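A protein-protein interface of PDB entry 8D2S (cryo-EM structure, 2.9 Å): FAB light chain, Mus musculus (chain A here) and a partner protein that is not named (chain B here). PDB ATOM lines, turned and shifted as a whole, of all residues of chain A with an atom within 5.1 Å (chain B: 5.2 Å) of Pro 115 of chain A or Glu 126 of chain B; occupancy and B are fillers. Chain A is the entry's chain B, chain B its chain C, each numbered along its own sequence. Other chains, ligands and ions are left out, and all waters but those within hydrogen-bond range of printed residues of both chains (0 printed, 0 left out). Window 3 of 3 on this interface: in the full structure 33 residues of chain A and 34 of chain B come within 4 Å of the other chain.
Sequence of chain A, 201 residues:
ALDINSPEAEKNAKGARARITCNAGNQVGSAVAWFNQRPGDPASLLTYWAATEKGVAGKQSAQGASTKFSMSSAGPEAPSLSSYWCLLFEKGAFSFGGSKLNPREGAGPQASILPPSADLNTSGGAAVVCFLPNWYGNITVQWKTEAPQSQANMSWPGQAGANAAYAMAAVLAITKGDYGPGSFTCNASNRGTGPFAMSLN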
ATOM      1  N   ILE A 113      -9.744  21.043   2.380  1.00  0.00           N
ATOM      2  CA  ILE A 113      -9.227  21.928   3.415  1.00  0.00           C
ATOM      3  C   ILE A 113      -7.875  22.476   2.968  1.00  0.00           C
ATOM      4  O   ILE A 113      -7.118  21.819   2.245  1.00  0.00           O
ATOM      5  CB  ILE A 113      -9.136  21.210   4.784  1.00  0.00           C
ATOM      6  CG1 ILE A 113      -8.990  22.221   5.924  1.00  0.00           C
ATOM      7  CG2 ILE A 113      -8.006  20.184   4.810  1.00  0.00           C
ATOM      8  CD1 ILE A 113      -9.109  21.610   7.300  1.00  0.00           C
ATOM      9  N   LEU A 114      -7.593  23.719   3.376  1.00  0.00           N
ATOM     10  CA  LEU A 114      -6.391  24.427   2.979  1.00  0.00           C
ATOM     11  C   LEU A 114      -5.821  25.129   4.208  1.00  0.00           C
ATOM     12  O   LEU A 114      -6.548  25.889   4.883  1.00  0.00           O
ATOM     13  CB  LEU A 114      -6.664  25.444   1.863  1.00  0.00           C
ATOM     14  CG  LEU A 114      -7.127  24.923   0.496  1.00  0.00           C
ATOM     15  CD1 LEU A 114      -8.641  24.782   0.425  1.00  0.00           C
ATOM     16  CD2 LEU A 114      -6.627  25.822  -0.622  1.00  0.00           C
ATOM     17  N   PRO A 115      -4.548  24.903   4.520  1.00  0.00           N
ATOM     18  CA  PRO A 115      -3.935  25.527   5.696  1.00  0.00           C
ATOM     19  C   PRO A 115      -3.594  26.982   5.427  1.00  0.00           C
ATOM     20  O   PRO A 115      -3.626  27.428   4.269  1.00  0.00           O
ATOM     21  CB  PRO A 115      -2.669  24.685   5.910  1.00  0.00           C
ATOM     22  CG  PRO A 115      -2.308  24.230   4.541  1.00  0.00           C
ATOM     23  CD  PRO A 115      -3.614  24.002   3.823  1.00  0.00           C
ATOM     24  N   PRO A 116      -3.288  27.760   6.469  1.00  0.00           N
ATOM     25  CA  PRO A 116      -2.840  29.141   6.250  1.00  0.00           C
ATOM     26  C   PRO A 116      -1.528  29.197   5.482  1.00  0.00           C
ATOM     27  O   PRO A 116      -0.657  28.337   5.626  1.00  0.00           O
ATOM     28  CB  PRO A 116      -2.675  29.690   7.671  1.00  0.00           C
ATOM     29  CG  PRO A 116      -3.565  28.844   8.506  1.00  0.00           C
ATOM     30  CD  PRO A 116      -3.515  27.480   7.898  1.00  0.00           C
ATOM     31  N   SER A 117      -1.394  30.233   4.659  1.00  0.00           N
ATOM     32  CA  SER A 117      -0.205  30.410   3.842  1.00  0.00           C
ATOM     33  C   SER A 117       0.938  30.992   4.671  1.00  0.00           C
ATOM     34  O   SER A 117       0.766  31.408   5.820  1.00  0.00           O
ATOM     35  CB  SER A 117      -0.508  31.311   2.646  1.00  0.00           C
ATOM     36  OG  SER A 117       0.652  31.518   1.860  1.00  0.00           O
ATOM     37  N   ALA A 127      -5.510  31.658   8.880  1.00  0.00           N
ATOM     38  CA  ALA A 127      -6.867  31.339   8.456  1.00  0.00           C
ATOM     39  C   ALA A 127      -6.860  29.996   7.742  1.00  0.00           C
ATOM     40  O   ALA A 127      -6.189  29.836   6.716  1.00  0.00           O
ATOM     41  CB  ALA A 127      -7.437  32.430   7.551  1.00  0.00           C
ATOM     42  N   VAL A 128      -7.605  29.039   8.283  1.00  0.00           N
ATOM     43  CA  VAL A 128      -7.764  27.722   7.675  1.00  0.00           C
ATOM     44  C   VAL A 128      -9.066  27.735   6.888  1.00  0.00           C
ATOM     45  O   VAL A 128     -10.125  28.056   7.439  1.00  0.00           O
ATOM     46  CB  VAL A 128      -7.761  26.608   8.732  1.00  0.00           C
ATOM     47  CG1 VAL A 128      -7.546  25.258   8.071  1.00  0.00           C
ATOM     48  CG2 VAL A 128      -6.695  26.874   9.780  1.00  0.00           C
ATOM     49  N   TYR A 179      -2.337  28.868  17.344  1.00  0.00           N
ATOM     50  CA  TYR A 179      -1.989  27.812  16.395  1.00  0.00           C
ATOM     51  C   TYR A 179      -1.160  26.724  17.066  1.00  0.00           C
ATOM     52  O   TYR A 179      -0.252  26.144  16.464  1.00  0.00           O
ATOM     53  CB  TYR A 179      -1.245  28.404  15.201  1.00  0.00           C
ATOM     54  CG  TYR A 179      -1.461  27.671  13.895  1.00  0.00           C
ATOM     55  CD1 TYR A 179      -2.630  27.844  13.166  1.00  0.00           C
ATOM     56  CD2 TYR A 179      -0.488  26.822  13.382  1.00  0.00           C
ATOM     57  CE1 TYR A 179      -2.830  27.183  11.969  1.00  0.00           C
ATOM     58  CE2 TYR A 179      -0.679  26.157  12.187  1.00  0.00           C
ATOM     59  CZ  TYR A 179      -1.851  26.341  11.485  1.00  0.00           C
ATOM     60  OH  TYR A 179      -2.044  25.680  10.295  1.00  0.00           O
ATOM     61  N   LEU A 200      -5.867  18.373   8.336  1.00  0.00           N
ATOM     62  CA  LEU A 200      -4.469  18.725   8.142  1.00  0.00           C
ATOM     63  C   LEU A 200      -3.775  18.747   9.496  1.00  0.00           C
ATOM     64  O   LEU A 200      -4.399  19.019  10.526  1.00  0.00           O
ATOM     65  CB  LEU A 200      -4.306  20.082   7.433  1.00  0.00           C
ATOM     66  CG  LEU A 200      -4.729  21.371   8.148  1.00  0.00           C
ATOM     67  CD1 LEU A 200      -3.534  22.092   8.765  1.00  0.00           C
ATOM     68  CD2 LEU A 200      -5.459  22.287   7.185  1.00  0.00           C
ATOM     69  N   PRO B 124      -2.229  33.225  -1.016  1.00  0.00           N
ATOM     70  CA  PRO B 124      -2.419  32.054  -1.897  1.00  0.00           C
ATOM     71  C   PRO B 124      -2.545  30.740  -1.129  1.00  0.00           C
ATOM     72  O   PRO B 124      -1.593  29.983  -0.932  1.00  0.00           O
ATOM     73  CB  PRO B 124      -1.164  32.093  -2.772  1.00  0.00           C
ATOM     74  CG  PRO B 124      -0.120  32.695  -1.887  1.00  0.00           C
ATOM     75  CD  PRO B 124      -0.827  33.677  -0.986  1.00  0.00           C
ATOM     76  N   VAL B 125      -3.762  30.458  -0.662  1.00  0.00           N
ATOM     77  CA  VAL B 125      -4.031  29.176  -0.021  1.00  0.00           C
ATOM     78  C   VAL B 125      -3.932  28.072  -1.064  1.00  0.00           C
ATOM     79  O   VAL B 125      -4.516  28.166  -2.152  1.00  0.00           O
ATOM     80  CB  VAL B 125      -5.404  29.188   0.669  1.00  0.00           C
ATOM     81  CG1 VAL B 125      -5.302  29.849   2.032  1.00  0.00           C
ATOM     82  CG2 VAL B 125      -6.425  29.912  -0.183  1.00  0.00           C
ATOM     83  N   GLU B 126      -3.184  27.020  -0.740  1.00  0.00           N
ATOM     84  CA  GLU B 126      -2.821  26.003  -1.713  1.00  0.00           C
ATOM     85  C   GLU B 126      -3.029  24.628  -1.089  1.00  0.00           C
ATOM     86  O   GLU B 126      -3.639  24.490  -0.023  1.00  0.00           O
ATOM     87  CB  GLU B 126      -1.376  26.204  -2.189  1.00  0.00           C
ATOM     88  N   ILE B 127      -2.510  23.603  -1.767  1.00  0.00           N
ATOM     89  CA  ILE B 127      -2.718  22.230  -1.329  1.00  0.00           C
ATOM     90  C   ILE B 127      -1.872  21.934  -0.094  1.00  0.00           C
ATOM     91  O   ILE B 127      -0.950  22.676   0.267  1.00  0.00           O
ATOM     92  CB  ILE B 127      -2.396  21.253  -2.469  1.00  0.00           C
ATOM     93  CG1 ILE B 127      -0.893  21.244  -2.751  1.00  0.00           C
ATOM     94  CG2 ILE B 127      -3.156  21.645  -3.721  1.00  0.00           C
ATOM     95  CD1 ILE B 127      -0.487  20.333  -3.890  1.00  0.00           C
ATOM     96  N   SER B 128      -2.199  20.823   0.564  1.00  0.00           N
ATOM     97  CA  SER B 128      -1.485  20.364   1.748  1.00  0.00           C
ATOM     98  C   SER B 128      -0.697  19.085   1.475  1.00  0.00           C
ATOM     99  O   SER B 128      -0.522  18.252   2.368  1.00  0.00           O
ATOM    100  CB  SER B 128      -2.456  20.155   2.909  1.00  0.00           C
ATOM    101  OG  SER B 128      -3.453  19.205   2.575  1.00  0.00           O
ATOM    102  N   LEU B 137      -7.607  24.720  -5.908  1.00  0.00           N
ATOM    103  CA  LEU B 137      -6.770  25.807  -5.436  1.00  0.00           C
ATOM    104  C   LEU B 137      -7.641  26.838  -4.722  1.00  0.00           C
ATOM    105  O   LEU B 137      -8.837  26.628  -4.501  1.00  0.00           O
ATOM    106  CB  LEU B 137      -5.996  26.417  -6.604  1.00  0.00           C
ATOM    107  CG  LEU B 137      -5.102  25.446  -7.377  1.00  0.00           C
ATOM    108  CD1 LEU B 137      -4.503  26.131  -8.593  1.00  0.00           C
ATOM    109  CD2 LEU B 137      -4.012  24.888  -6.477  1.00  0.00           C
ATOM    110  N   VAL B 200       0.246  30.887  -7.132  1.00  0.00           N
ATOM    111  CA  VAL B 200      -0.011  29.836  -6.156  1.00  0.00           C
ATOM    112  C   VAL B 200       1.031  28.745  -6.353  1.00  0.00           C
ATOM    113  O   VAL B 200       1.086  28.110  -7.413  1.00  0.00           O
ATOM    114  CB  VAL B 200      -1.434  29.274  -6.299  1.00  0.00           C
ATOM    115  CG1 VAL B 200      -1.651  28.124  -5.331  1.00  0.00           C
ATOM    116  CG2 VAL B 200      -2.462  30.371  -6.069  1.00  0.00           C
ATOM    117  N   ALA B 201       1.862  28.529  -5.339  1.00  0.00           N
ATOM    118  CA  ALA B 201       2.921  27.535  -5.393  1.00  0.00           C
ATOM    119  C   ALA B 201       2.494  26.259  -4.675  1.00  0.00           C
ATOM    120  O   ALA B 201       1.437  26.187  -4.045  1.00  0.00           O
ATOM    121  CB  ALA B 201       4.210  28.089  -4.782  1.00  0.00           C
ATOM    122  N   ALA B 203       2.885  23.090  -1.895  1.00  0.00           N
ATOM    123  CA  ALA B 203       3.115  22.950  -0.453  1.00  0.00           C
ATOM    124  C   ALA B 203       2.864  24.249   0.310  1.00  0.00           C
ATOM    125  O   ALA B 203       2.022  24.301   1.206  1.00  0.00           O
ATOM    126  CB  ALA B 203       4.532  22.441  -0.184  1.00  0.00           C
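CD2 of Leu 114 of chain A touches O of Val 125 of chain B (3.5 Å). Leu 114 of chain A touches Glu 126 of chain B (CD2 to O, 3.3 Å). Val 125 of chain B touches Pro 115 of chain A (CG1 to O, 3.7 Å). Pro 115 of chain A touches Glu 126 of chain B (CD to O, 3.9 Å). Ser 117 of chain A touches Pro 124 of chain B.
Of the printed residues of chain B, Ser 117 of chain A touches Pro 124. Printed residues of chain A within 4 Å of Val 125 of chain B: Leu 114 (3.5 Å) and Pro 115 (3.7 Å). Of chain A, only Leu 114 (3.3 Å) and Pro 115 (3.9 Å) come within 4 Å of Glu 126 of chain B.
Of the 9 printed residues of chain A, 3 touch a printed residue of chain B. Hydrophobic or aromatic side chains of chain A that line the printed part of chain B: Leu 114 and Pro 115. Hydrophobic or aromatic side chains of chain B within 4 Å of the printed part of chain A: Pro 124 and Val 125. Among the printed residues, 5 pairs touch across the chains.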
